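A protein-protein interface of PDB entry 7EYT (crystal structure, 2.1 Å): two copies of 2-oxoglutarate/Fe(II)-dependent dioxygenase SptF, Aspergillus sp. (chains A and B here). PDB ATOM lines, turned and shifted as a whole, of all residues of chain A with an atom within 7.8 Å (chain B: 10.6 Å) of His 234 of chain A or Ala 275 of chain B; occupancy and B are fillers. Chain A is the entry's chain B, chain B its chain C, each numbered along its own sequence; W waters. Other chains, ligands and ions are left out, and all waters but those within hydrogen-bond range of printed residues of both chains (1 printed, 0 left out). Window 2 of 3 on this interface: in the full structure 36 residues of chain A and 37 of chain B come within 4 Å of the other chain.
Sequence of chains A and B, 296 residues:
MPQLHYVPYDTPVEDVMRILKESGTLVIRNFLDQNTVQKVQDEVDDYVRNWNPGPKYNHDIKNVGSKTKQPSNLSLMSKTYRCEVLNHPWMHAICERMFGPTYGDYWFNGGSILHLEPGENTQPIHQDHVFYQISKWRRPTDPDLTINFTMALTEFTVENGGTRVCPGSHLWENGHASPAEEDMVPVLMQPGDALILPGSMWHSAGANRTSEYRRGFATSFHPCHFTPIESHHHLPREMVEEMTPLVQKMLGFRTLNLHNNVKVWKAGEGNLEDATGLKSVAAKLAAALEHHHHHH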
ATOM      1  N   TYR A  47       6.596  -2.937  16.116  1.00  0.00           N
ATOM      2  CA  TYR A  47       7.089  -3.976  17.014  1.00  0.00           C
ATOM      3  C   TYR A  47       6.455  -3.865  18.395  1.00  0.00           C
ATOM      4  O   TYR A  47       5.919  -4.846  18.921  1.00  0.00           O
ATOM      5  CB  TYR A  47       8.614  -3.901  17.121  1.00  0.00           C
ATOM      6  CG  TYR A  47       9.209  -4.878  18.114  1.00  0.00           C
ATOM      7  CD1 TYR A  47       9.581  -6.157  17.723  1.00  0.00           C
ATOM      8  CD2 TYR A  47       9.398  -4.520  19.445  1.00  0.00           C
ATOM      9  CE1 TYR A  47      10.124  -7.052  18.628  1.00  0.00           C
ATOM     10  CE2 TYR A  47       9.938  -5.407  20.356  1.00  0.00           C
ATOM     11  CZ  TYR A  47      10.300  -6.670  19.943  1.00  0.00           C
ATOM     12  OH  TYR A  47      10.839  -7.555  20.850  1.00  0.00           O
ATOM     13  N   SER A  72      13.023  -3.541  22.913  1.00  0.00           N
ATOM     14  CA  SER A  72      14.244  -4.324  22.991  1.00  0.00           C
ATOM     15  C   SER A  72      15.349  -3.601  22.214  1.00  0.00           C
ATOM     16  O   SER A  72      15.323  -2.363  22.109  1.00  0.00           O
ATOM     17  CB  SER A  72      13.958  -5.737  22.488  1.00  0.00           C
ATOM     18  OG  SER A  72      15.098  -6.566  22.627  1.00  0.00           O
ATOM     19  N   ASN A  73      16.308  -4.357  21.684  1.00  0.00           N
ATOM     20  CA  ASN A  73      17.377  -3.757  20.899  1.00  0.00           C
ATOM     21  C   ASN A  73      16.825  -3.172  19.604  1.00  0.00           C
ATOM     22  O   ASN A  73      15.871  -3.691  19.017  1.00  0.00           O
ATOM     23  CB  ASN A  73      18.458  -4.790  20.581  1.00  0.00           C
ATOM     24  CG  ASN A  73      19.006  -5.462  21.823  1.00  0.00           C
ATOM     25  OD1 ASN A  73      18.264  -6.085  22.581  1.00  0.00           O
ATOM     26  ND2 ASN A  73      20.312  -5.342  22.037  1.00  0.00           N
ATOM     27  N   LEU A  74      17.441  -2.073  19.160  1.00  0.00           N
ATOM     28  CA  LEU A  74      17.015  -1.446  17.914  1.00  0.00           C
ATOM     29  C   LEU A  74      17.226  -2.372  16.723  1.00  0.00           C
ATOM     30  O   LEU A  74      16.438  -2.345  15.771  1.00  0.00           O
ATOM     31  CB  LEU A  74      17.762  -0.128  17.705  1.00  0.00           C
ATOM     32  CG  LEU A  74      16.989   1.151  18.034  1.00  0.00           C
ATOM     33  CD1 LEU A  74      17.847   2.381  17.783  1.00  0.00           C
ATOM     34  CD2 LEU A  74      15.695   1.222  17.233  1.00  0.00           C
ATOM     35  N   SER A  75      18.272  -3.200  16.760  1.00  0.00           N
ATOM     36  CA  SER A  75      18.518  -4.124  15.658  1.00  0.00           C
ATOM     37  C   SER A  75      17.511  -5.266  15.644  1.00  0.00           C
ATOM     38  O   SER A  75      17.261  -5.856  14.588  1.00  0.00           O
ATOM     39  CB  SER A  75      19.944  -4.667  15.737  1.00  0.00           C
ATOM     40  OG  SER A  75      20.887  -3.610  15.707  1.00  0.00           O
ATOM     41  N   LEU A  76      16.926  -5.591  16.798  1.00  0.00           N
ATOM     42  CA  LEU A  76      15.877  -6.601  16.837  1.00  0.00           C
ATOM     43  C   LEU A  76      14.532  -6.039  16.394  1.00  0.00           C
ATOM     44  O   LEU A  76      13.735  -6.759  15.784  1.00  0.00           O
ATOM     45  CB  LEU A  76      15.767  -7.193  18.245  1.00  0.00           C
ATOM     46  CG  LEU A  76      14.610  -8.156  18.533  1.00  0.00           C
ATOM     47  CD1 LEU A  76      14.681  -9.394  17.650  1.00  0.00           C
ATOM     48  CD2 LEU A  76      14.582  -8.550  20.002  1.00  0.00           C
ATOM     49  N   GLU A 230      25.039  -3.390  24.789  1.00  0.00           N
ATOM     50  CA  GLU A 230      23.957  -4.291  24.428  1.00  0.00           C
ATOM     51  C   GLU A 230      24.508  -5.614  23.914  1.00  0.00           C
ATOM     52  O   GLU A 230      25.497  -5.644  23.175  1.00  0.00           O
ATOM     53  CB  GLU A 230      23.058  -3.666  23.357  1.00  0.00           C
ATOM     54  CG  GLU A 230      22.187  -2.520  23.844  1.00  0.00           C
ATOM     55  CD  GLU A 230      21.635  -1.696  22.699  1.00  0.00           C
ATOM     56  OE1 GLU A 230      21.176  -2.294  21.704  1.00  0.00           O
ATOM     57  OE2 GLU A 230      21.688  -0.450  22.778  1.00  0.00           O
ATOM     58  N   SER A 231      23.858  -6.702  24.311  1.00  0.00           N
ATOM     59  CA  SER A 231      24.089  -8.012  23.726  1.00  0.00           C
ATOM     60  C   SER A 231      22.934  -8.349  22.795  1.00  0.00           C
ATOM     61  O   SER A 231      21.777  -8.022  23.080  1.00  0.00           O
ATOM     62  CB  SER A 231      24.222  -9.087  24.805  1.00  0.00           C
ATOM     63  OG  SER A 231      23.998 -10.375  24.262  1.00  0.00           O
ATOM     64  N   HIS A 232      23.252  -8.997  21.675  1.00  0.00           N
ATOM     65  CA  HIS A 232      22.245  -9.428  20.714  1.00  0.00           C
ATOM     66  C   HIS A 232      22.144 -10.947  20.636  1.00  0.00           C
ATOM     67  O   HIS A 232      21.671 -11.487  19.631  1.00  0.00           O
ATOM     68  CB  HIS A 232      22.542  -8.830  19.339  1.00  0.00           C
ATOM     69  CG  HIS A 232      22.500  -7.334  19.315  1.00  0.00           C
ATOM     70  ND1 HIS A 232      23.505  -6.553  19.845  1.00  0.00           N
ATOM     71  CD2 HIS A 232      21.568  -6.475  18.839  1.00  0.00           C
ATOM     72  CE1 HIS A 232      23.197  -5.278  19.692  1.00  0.00           C
ATOM     73  NE2 HIS A 232      22.027  -5.202  19.083  1.00  0.00           N
ATOM     74  N   HIS A 233      22.571 -11.644  21.692  1.00  0.00           N
ATOM     75  CA  HIS A 233      22.540 -13.102  21.717  1.00  0.00           C
ATOM     76  C   HIS A 233      21.124 -13.660  21.649  1.00  0.00           C
ATOM     77  O   HIS A 233      20.941 -14.806  21.225  1.00  0.00           O
ATOM     78  CB  HIS A 233      23.245 -13.603  22.977  1.00  0.00           C
ATOM     79  CG  HIS A 233      23.349 -15.094  23.060  1.00  0.00           C
ATOM     80  ND1 HIS A 233      23.923 -15.858  22.068  1.00  0.00           N
ATOM     81  CD2 HIS A 233      22.957 -15.961  24.023  1.00  0.00           C
ATOM     82  CE1 HIS A 233      23.873 -17.133  22.412  1.00  0.00           C
ATOM     83  NE2 HIS A 233      23.294 -17.222  23.596  1.00  0.00           N
ATOM     84  N   HIS A 234      20.122 -12.882  22.050  1.00  0.00           N
ATOM     85  CA  HIS A 234      18.737 -13.336  22.046  1.00  0.00           C
ATOM     86  C   HIS A 234      18.070 -13.214  20.682  1.00  0.00           C
ATOM     87  O   HIS A 234      16.900 -13.587  20.549  1.00  0.00           O
ATOM     88  CB  HIS A 234      17.928 -12.551  23.085  1.00  0.00           C
ATOM     89  CG  HIS A 234      17.917 -11.072  22.850  1.00  0.00           C
ATOM     90  ND1 HIS A 234      19.062 -10.305  22.871  1.00  0.00           N
ATOM     91  CD2 HIS A 234      16.898 -10.219  22.588  1.00  0.00           C
ATOM     92  CE1 HIS A 234      18.749  -9.044  22.632  1.00  0.00           C
ATOM     93  NE2 HIS A 234      17.442  -8.964  22.457  1.00  0.00           N
ATOM     94  N   LEU A 235      18.779 -12.720  19.671  1.00  0.00           N
ATOM     95  CA  LEU A 235      18.161 -12.481  18.378  1.00  0.00           C
ATOM     96  C   LEU A 235      17.892 -13.802  17.659  1.00  0.00           C
ATOM     97  O   LEU A 235      18.656 -14.761  17.797  1.00  0.00           O
ATOM     98  CB  LEU A 235      19.053 -11.588  17.520  1.00  0.00           C
ATOM     99  CG  LEU A 235      18.759 -10.085  17.568  1.00  0.00           C
ATOM    100  CD1 LEU A 235      18.771  -9.558  18.997  1.00  0.00           C
ATOM    101  CD2 LEU A 235      19.748  -9.314  16.705  1.00  0.00           C
ATOM    102  N   PRO A 236      16.805 -13.878  16.890  1.00  0.00           N
ATOM    103  CA  PRO A 236      16.486 -15.127  16.185  1.00  0.00           C
ATOM    104  C   PRO A 236      17.552 -15.478  15.157  1.00  0.00           C
ATOM    105  O   PRO A 236      18.200 -14.606  14.573  1.00  0.00           O
ATOM    106  CB  PRO A 236      15.140 -14.826  15.513  1.00  0.00           C
ATOM    107  CG  PRO A 236      14.592 -13.635  16.237  1.00  0.00           C
ATOM    108  CD  PRO A 236      15.780 -12.843  16.678  1.00  0.00           C
ATOM    109  N   ARG A 237      17.724 -16.785  14.940  1.00  0.00           N
ATOM    110  CA  ARG A 237      18.768 -17.265  14.038  1.00  0.00           C
ATOM    111  C   ARG A 237      18.534 -16.807  12.604  1.00  0.00           C
ATOM    112  O   ARG A 237      19.497 -16.541  11.874  1.00  0.00           O
ATOM    113  CB  ARG A 237      18.852 -18.790  14.105  1.00  0.00           C
ATOM    114  CG  ARG A 237      19.937 -19.398  13.229  1.00  0.00           C
ATOM    115  CD  ARG A 237      19.443 -20.658  12.536  1.00  0.00           C
ATOM    116  NE  ARG A 237      18.406 -21.337  13.305  1.00  0.00           N
ATOM    117  CZ  ARG A 237      17.232 -21.713  12.814  1.00  0.00           C
ATOM    118  NH1 ARG A 237      16.907 -21.487  11.551  1.00  0.00           N
ATOM    119  NH2 ARG A 237      16.364 -22.331  13.609  1.00  0.00           N
ATOM    120  N   MET A 239      17.366 -13.994  11.648  1.00  0.00           N
ATOM    121  CA  MET A 239      17.781 -12.602  11.522  1.00  0.00           C
ATOM    122  C   MET A 239      19.295 -12.490  11.412  1.00  0.00           C
ATOM    123  O   MET A 239      19.811 -11.657  10.657  1.00  0.00           O
ATOM    124  CB  MET A 239      17.275 -11.804  12.719  1.00  0.00           C
ATOM    125  CG  MET A 239      16.177 -10.827  12.381  1.00  0.00           C
ATOM    126  SD  MET A 239      15.357 -10.223  13.862  1.00  0.00           S
ATOM    127  CE  MET A 239      16.726  -9.383  14.644  1.00  0.00           C
ATOM    128  N   VAL A 240      20.022 -13.318  12.162  1.00  0.00           N
ATOM    129  CA  VAL A 240      21.480 -13.297  12.102  1.00  0.00           C
ATOM    130  C   VAL A 240      21.959 -13.716  10.719  1.00  0.00           C
ATOM    131  O   VAL A 240      22.901 -13.133  10.167  1.00  0.00           O
ATOM    132  CB  VAL A 240      22.071 -14.195  13.204  1.00  0.00           C
ATOM    133  CG1 VAL A 240      23.586 -14.062  13.248  1.00  0.00           C
ATOM    134  CG2 VAL A 240      21.456 -13.853  14.555  1.00  0.00           C
ATOM    135  N   PHE A 253      28.362 -11.657  16.598  1.00  0.00           N
ATOM    136  CA  PHE A 253      28.203 -13.024  16.122  1.00  0.00           C
ATOM    137  C   PHE A 253      29.449 -13.556  15.428  1.00  0.00           C
ATOM    138  O   PHE A 253      29.418 -14.668  14.892  1.00  0.00           O
ATOM    139  CB  PHE A 253      27.004 -13.117  15.177  1.00  0.00           C
ATOM    140  CG  PHE A 253      25.704 -12.716  15.811  1.00  0.00           C
ATOM    141  CD1 PHE A 253      25.116 -13.514  16.778  1.00  0.00           C
ATOM    142  CD2 PHE A 253      25.073 -11.538  15.444  1.00  0.00           C
ATOM    143  CE1 PHE A 253      23.920 -13.148  17.366  1.00  0.00           C
ATOM    144  CE2 PHE A 253      23.876 -11.165  16.029  1.00  0.00           C
ATOM    145  CZ  PHE A 253      23.300 -11.971  16.991  1.00  0.00           C
ATOM    146  N   HIS B 233      28.822 -18.679  23.095  1.00  0.00           N
ATOM    147  CA  HIS B 233      27.490 -18.723  22.508  1.00  0.00           C
ATOM    148  C   HIS B 233      27.324 -19.863  21.512  1.00  0.00           C
ATOM    149  O   HIS B 233      26.233 -20.023  20.953  1.00  0.00           O
ATOM    150  CB  HIS B 233      27.177 -17.381  21.845  1.00  0.00           C
ATOM    151  CG  HIS B 233      27.105 -16.240  22.813  1.00  0.00           C
ATOM    152  ND1 HIS B 233      26.984 -14.926  22.414  1.00  0.00           N
ATOM    153  CD2 HIS B 233      27.139 -16.220  24.167  1.00  0.00           C
ATOM    154  CE1 HIS B 233      26.944 -14.147  23.479  1.00  0.00           C
ATOM    155  NE2 HIS B 233      27.038 -14.906  24.556  1.00  0.00           N
ATOM    156  N   ARG B 237      22.294 -25.374  24.306  1.00  0.00           N
ATOM    157  CA  ARG B 237      21.420 -24.714  25.273  1.00  0.00           C
ATOM    158  C   ARG B 237      21.309 -25.516  26.564  1.00  0.00           C
ATOM    159  O   ARG B 237      21.348 -24.946  27.661  1.00  0.00           O
ATOM    160  CB  ARG B 237      20.037 -24.488  24.656  1.00  0.00           C
ATOM    161  CG  ARG B 237      18.880 -24.610  25.639  1.00  0.00           C
ATOM    162  CD  ARG B 237      17.587 -24.069  25.051  1.00  0.00           C
ATOM    163  NE  ARG B 237      16.486 -24.137  26.005  1.00  0.00           N
ATOM    164  CZ  ARG B 237      15.233 -23.797  25.732  1.00  0.00           C
ATOM    165  NH1 ARG B 237      14.881 -23.360  24.533  1.00  0.00           N
ATOM    166  NH2 ARG B 237      14.311 -23.898  26.684  1.00  0.00           N
ATOM    167  N   GLY B 252      29.167 -15.553  29.816  1.00  0.00           N
ATOM    168  CA  GLY B 252      28.591 -14.589  28.898  1.00  0.00           C
ATOM    169  C   GLY B 252      27.112 -14.728  28.611  1.00  0.00           C
ATOM    170  O   GLY B 252      26.658 -14.254  27.563  1.00  0.00           O
ATOM    171  N   PHE B 253      26.341 -15.344  29.503  1.00  0.00           N
ATOM    172  CA  PHE B 253      24.918 -15.552  29.276  1.00  0.00           C
ATOM    173  C   PHE B 253      24.036 -14.644  30.121  1.00  0.00           C
ATOM    174  O   PHE B 253      22.808 -14.773  30.068  1.00  0.00           O
ATOM    175  CB  PHE B 253      24.553 -17.018  29.539  1.00  0.00           C
ATOM    176  CG  PHE B 253      25.309 -17.991  28.679  1.00  0.00           C
ATOM    177  CD1 PHE B 253      24.987 -18.149  27.340  1.00  0.00           C
ATOM    178  CD2 PHE B 253      26.350 -18.737  29.206  1.00  0.00           C
ATOM    179  CE1 PHE B 253      25.683 -19.040  26.545  1.00  0.00           C
ATOM    180  CE2 PHE B 253      27.050 -19.631  28.416  1.00  0.00           C
ATOM    181  CZ  PHE B 253      26.717 -19.782  27.085  1.00  0.00           C
ATOM    182  N   ARG B 254      24.620 -13.727  30.888  1.00  0.00           N
ATOM    183  CA  ARG B 254      23.852 -12.853  31.758  1.00  0.00           C
ATOM    184  C   ARG B 254      24.412 -11.439  31.685  1.00  0.00           C
ATOM    185  O   ARG B 254      25.578 -11.224  31.347  1.00  0.00           O
ATOM    186  CB  ARG B 254      23.854 -13.361  33.207  1.00  0.00           C
ATOM    187  CG  ARG B 254      22.783 -14.404  33.476  1.00  0.00           C
ATOM    188  CD  ARG B 254      23.106 -15.269  34.682  1.00  0.00           C
ATOM    189  NE  ARG B 254      22.088 -16.294  34.879  1.00  0.00           N
ATOM    190  CZ  ARG B 254      20.988 -16.128  35.599  1.00  0.00           C
ATOM    191  NH1 ARG B 254      20.744 -14.997  36.241  1.00  0.00           N
ATOM    192  NH2 ARG B 254      20.106 -17.121  35.676  1.00  0.00           N
ATOM    193  N   THR B 255      23.552 -10.476  32.005  1.00  0.00           N
ATOM    194  CA  THR B 255      23.943  -9.074  31.991  1.00  0.00           C
ATOM    195  C   THR B 255      24.910  -8.780  33.133  1.00  0.00           C
ATOM    196  O   THR B 255      24.791  -9.337  34.228  1.00  0.00           O
ATOM    197  CB  THR B 255      22.698  -8.186  32.092  1.00  0.00           C
ATOM    198  OG1 THR B 255      21.904  -8.348  30.911  1.00  0.00           O
ATOM    199  CG2 THR B 255      23.072  -6.718  32.237  1.00  0.00           C
ATOM    200  N   TRP B 265      26.232  -5.555  28.380  1.00  0.00           N
ATOM    201  CA  TRP B 265      25.806  -6.876  27.913  1.00  0.00           C
ATOM    202  C   TRP B 265      24.316  -7.092  28.185  1.00  0.00           C
ATOM    203  O   TRP B 265      23.902  -8.095  28.771  1.00  0.00           O
ATOM    204  CB  TRP B 265      26.656  -7.981  28.552  1.00  0.00           C
ATOM    205  CG  TRP B 265      26.861  -9.203  27.707  1.00  0.00           C
ATOM    206  CD1 TRP B 265      26.654 -10.500  28.085  1.00  0.00           C
ATOM    207  CD2 TRP B 265      27.330  -9.251  26.352  1.00  0.00           C
ATOM    208  NE1 TRP B 265      26.958 -11.349  27.050  1.00  0.00           N
ATOM    209  CE2 TRP B 265      27.373 -10.608  25.975  1.00  0.00           C
ATOM    210  CE3 TRP B 265      27.711  -8.279  25.421  1.00  0.00           C
ATOM    211  CZ2 TRP B 265      27.783 -11.018  24.707  1.00  0.00           C
ATOM    212  CZ3 TRP B 265      28.117  -8.688  24.163  1.00  0.00           C
ATOM    213  CH2 TRP B 265      28.149 -10.045  23.818  1.00  0.00           C
ATOM    214  N   LYS B 266      23.506  -6.129  27.752  1.00  0.00           N
ATOM    215  CA  LYS B 266      22.071  -6.119  27.995  1.00  0.00           C
ATOM    216  C   LYS B 266      21.298  -6.531  26.748  1.00  0.00           C
ATOM    217  O   LYS B 266      21.777  -6.415  25.617  1.00  0.00           O
ATOM    218  CB  LYS B 266      21.603  -4.731  28.437  1.00  0.00           C
ATOM    219  CG  LYS B 266      22.278  -4.185  29.678  1.00  0.00           C
ATOM    220  CD  LYS B 266      21.684  -2.834  30.045  1.00  0.00           C
ATOM    221  CE  LYS B 266      22.091  -1.758  29.052  1.00  0.00           C
ATOM    222  NZ  LYS B 266      21.375  -0.475  29.303  1.00  0.00           N
ATOM    223  N   ALA B 267      20.075  -7.004  26.972  1.00  0.00           N
ATOM    224  CA  ALA B 267      19.130  -7.307  25.900  1.00  0.00           C
ATOM    225  C   ALA B 267      18.135  -6.155  25.842  1.00  0.00           C
ATOM    226  O   ALA B 267      17.147  -6.134  26.580  1.00  0.00           O
ATOM    227  CB  ALA B 267      18.436  -8.643  26.141  1.00  0.00           C
ATOM    228  N   GLY B 268      18.398  -5.193  24.962  1.00  0.00           N
ATOM    229  CA  GLY B 268      17.630  -3.966  24.945  1.00  0.00           C
ATOM    230  C   GLY B 268      17.954  -3.119  26.157  1.00  0.00           C
ATOM    231  O   GLY B 268      19.102  -2.704  26.341  1.00  0.00           O
ATOM    232  N   GLU B 269      16.951  -2.862  26.997  1.00  0.00           N
ATOM    233  CA  GLU B 269      17.175  -2.196  28.273  1.00  0.00           C
ATOM    234  C   GLU B 269      17.184  -3.161  29.451  1.00  0.00           C
ATOM    235  O   GLU B 269      17.755  -2.830  30.497  1.00  0.00           O
ATOM    236  CB  GLU B 269      16.107  -1.121  28.511  1.00  0.00           C
ATOM    237  N   GLY B 270      16.575  -4.336  29.306  1.00  0.00           N
ATOM    238  CA  GLY B 270      16.534  -5.323  30.363  1.00  0.00           C
ATOM    239  C   GLY B 270      17.745  -6.236  30.350  1.00  0.00           C
ATOM    240  O   GLY B 270      18.759  -5.976  29.699  1.00  0.00           O
ATOM    241  N   ASN B 271      17.622  -7.336  31.088  1.00  0.00           N
ATOM    242  CA  ASN B 271      18.713  -8.284  31.249  1.00  0.00           C
ATOM    243  C   ASN B 271      18.716  -9.312  30.123  1.00  0.00           C
ATOM    244  O   ASN B 271      17.669  -9.671  29.575  1.00  0.00           O
ATOM    245  CB  ASN B 271      18.612  -8.994  32.600  1.00  0.00           C
ATOM    246  CG  ASN B 271      18.973  -8.088  33.762  1.00  0.00           C
ATOM    247  OD1 ASN B 271      19.845  -7.226  33.644  1.00  0.00           O
ATOM    248  ND2 ASN B 271      18.302  -8.277  34.892  1.00  0.00           N
ATOM    249  N   LEU B 272      19.916  -9.788  29.783  1.00  0.00           N
ATOM    250  CA  LEU B 272      20.048 -10.782  28.724  1.00  0.00           C
ATOM    251  C   LEU B 272      19.408 -12.108  29.115  1.00  0.00           C
ATOM    252  O   LEU B 272      18.842 -12.799  28.260  1.00  0.00           O
ATOM    253  CB  LEU B 272      21.523 -10.981  28.374  1.00  0.00           C
ATOM    254  CG  LEU B 272      21.835 -11.998  27.275  1.00  0.00           C
ATOM    255  CD1 LEU B 272      21.295 -11.526  25.931  1.00  0.00           C
ATOM    256  CD2 LEU B 272      23.334 -12.267  27.195  1.00  0.00           C
ATOM    257  N   GLU B 273      19.481 -12.477  30.397  1.00  0.00           N
ATOM    258  CA  GLU B 273      18.871 -13.719  30.855  1.00  0.00           C
ATOM    259  C   GLU B 273      17.353 -13.687  30.759  1.00  0.00           C
ATOM    260  O   GLU B 273      16.729 -14.749  30.655  1.00  0.00           O
ATOM    261  CB  GLU B 273      19.293 -14.012  32.296  1.00  0.00           C
ATOM    262  CG  GLU B 273      19.083 -12.853  33.257  1.00  0.00           C
ATOM    263  CD  GLU B 273      20.341 -12.032  33.467  1.00  0.00           C
ATOM    264  OE1 GLU B 273      20.862 -11.479  32.475  1.00  0.00           O
ATOM    265  OE2 GLU B 273      20.812 -11.948  34.621  1.00  0.00           O
ATOM    266  N   ASP B 274      16.746 -12.500  30.790  1.00  0.00           N
ATOM    267  CA  ASP B 274      15.293 -12.412  30.680  1.00  0.00           C
ATOM    268  C   ASP B 274      14.832 -12.664  29.250  1.00  0.00           C
ATOM    269  O   ASP B 274      13.869 -13.404  29.024  1.00  0.00           O
ATOM    270  CB  ASP B 274      14.810 -11.047  31.166  1.00  0.00           C
ATOM    271  CG  ASP B 274      15.050 -10.833  32.647  1.00  0.00           C
ATOM    272  OD1 ASP B 274      14.827 -11.779  33.431  1.00  0.00           O
ATOM    273  OD2 ASP B 274      15.465  -9.719  33.026  1.00  0.00           O
ATOM    274  N   ALA B 275      15.510 -12.058  28.272  1.00  0.00           N
ATOM    275  CA  ALA B 275      15.129 -12.221  26.875  1.00  0.00           C
ATOM    276  C   ALA B 275      15.401 -13.623  26.347  1.00  0.00           C
ATOM    277  O   ALA B 275      14.880 -13.975  25.283  1.00  0.00           O
ATOM    278  CB  ALA B 275      15.862 -11.196  26.009  1.00  0.00           C
ATOM    279  N   THR B 276      16.193 -14.428  27.058  1.00  0.00           N
ATOM    280  CA  THR B 276      16.505 -15.782  26.627  1.00  0.00           C
ATOM    281  C   THR B 276      15.773 -16.859  27.414  1.00  0.00           C
ATOM    282  O   THR B 276      15.724 -18.006  26.955  1.00  0.00           O
ATOM    283  CB  THR B 276      18.016 -16.041  26.730  1.00  0.00           C
ATOM    284  OG1 THR B 276      18.494 -15.594  28.005  1.00  0.00           O
ATOM    285  CG2 THR B 276      18.758 -15.299  25.628  1.00  0.00           C
ATOM    286  N   GLY B 277      15.210 -16.528  28.574  1.00  0.00           N
ATOM    287  CA  GLY B 277      14.503 -17.505  29.377  1.00  0.00           C
ATOM    288  C   GLY B 277      15.424 -18.418  30.161  1.00  0.00           C
ATOM    289  O   GLY B 277      15.243 -19.640  30.167  1.00  0.00           O
ATOM    290  N   LEU B 278      16.418 -17.837  30.827  1.00  0.00           N
ATOM    291  CA  LEU B 278      17.352 -18.611  31.636  1.00  0.00           C
ATOM    292  C   LEU B 278      16.939 -18.601  33.104  1.00  0.00           C
ATOM    293  O   LEU B 278      16.214 -17.710  33.548  1.00  0.00           O
ATOM    294  CB  LEU B 278      18.774 -18.068  31.485  1.00  0.00           C
ATOM    295  CG  LEU B 278      19.706 -18.847  30.555  1.00  0.00           C
ATOM    296  CD1 LEU B 278      21.106 -18.251  30.580  1.00  0.00           C
ATOM    297  CD2 LEU B 278      19.735 -20.322  30.927  1.00  0.00           C
HETATM  298  O   HOH W   1      16.175 -15.802  22.690  1.00  0.00           O
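The backbone NH of Ser 231 of chain A is in hydrogen-bond range of the backbone carbonyl oxygen of Lys 266 of chain B, at 2.5 Å.
OD1 of Asn 73 of chain A is in hydrogen-bond range of N of Gly 268 of chain B, 2.5 Å away.
A ring nitrogen (ND1) of His 233 of chain A lies within hydrogen-bond range of a ring nitrogen (ND1) of His 233 of chain B, 3.2 Å away.
O of Gly 252 of chain B is in hydrogen-bond range of NE1 of Trp 265 of chain B (3.0 Å).
The side-chain carboxylate (OE1) of Glu 230 of chain A sits at hydrogen-bond distance from the side-chain amide nitrogen (ND2) of Asn 73 of chain A, 3.2 Å away.
NE2 of His 234 of chain A sits at hydrogen-bond distance from OD1 of Asn 73 of chain A (3.0 Å).
The backbone carbonyl oxygen of Ser 231 of chain A sits at hydrogen-bond distance from the side-chain amide nitrogen of Asn 73 of chain A, at 3.2 Å.
The side-chain hydroxyl of Ser 72 of chain A lies within hydrogen-bond range of a ring nitrogen (NE2) of His 234 of chain A (3.4 Å).
The side-chain hydroxyl (OG1) of Thr 276 of chain B lies within hydrogen-bond range of the backbone carbonyl oxygen (O) of Glu 273 of chain B, 3.3 Å away.
C of Ser 72 of chain A touches CA of Gly 268 of chain B, 3.6 Å away.
Asn 73 of chain A touches Ala 267 of chain B (OD1 to C, 3.3 Å).
Lys 266 of chain B touches Glu 230 of chain A (O to CA, 3.3 Å).
Gly 268 of chain B touches Glu 230 of chain A (O to CG, 3.97 Å).
O of Ser 231 of chain A touches CA of Ala 267 of chain B (3.9 Å).
Leu 272 of chain B touches Ser 231 of chain A (CD1 to OG, 3.4 Å).
Ala 267 of chain B touches His 234 of chain A.
His 234 of chain A touches Leu 272 of chain B (ND1 to CD1, 3.98 Å).
Ala 275 of chain B touches His 234 of chain A (CB to CD2, 3.7 Å).
Thr 276 of chain B touches His 234 of chain A (CG2 to CB, 3.8 Å).
Of the printed residues of chain B, Asn 73 of chain A touches Ala 267 and Gly 268.
Of the printed residues of chain B, Glu 230 of chain A touches Lys 266 and Gly 268.
Ser 231 of chain A touches just these residues of chain B: Trp 265, Lys 266, Ala 267 and Leu 272.
No residue of chain B comes within 4 Å of His 232 of chain A.
Of chain B, only His 233 (3.2 Å) comes within 4 Å of His 233 of chain A.
Of the printed residues of chain B, His 234 of chain A touches Ala 267, Leu 272, Ala 275 and Thr 276.
No residue of chain B comes within 4 Å of Leu 235 of chain A.
No residue of chain B comes within 4 Å of Pro 236 of chain A.
Of the printed residues of chain A, Ala 267 of chain B touches Asn 73, Ser 231 and His 234.
Ala 275 of chain B touches just one residue of chain A: His 234.
The nearest printed residue of chain B that does not touch His 234 of chain A is Gly 268 of chain B (4.5 Å).
Hydrophobic or aromatic side chains of chain A that line the printed part of chain B: His 233 and His 234.
Among the printed residues, no Asp or Glu carboxylate lies within 4 Å of a Lys or Arg side-chain nitrogen of the other chain.
His 233 of chain A touches its own counterpart, His 233 of chain B.
3 positions are printed for both chains.
Of the 14 pairs that touch across the chains among the printed residues, 1 has its exchanged pair printed and touching as well.
Water W1 bridges O of His 234 of chain A and O of Ala 275 of chain B.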
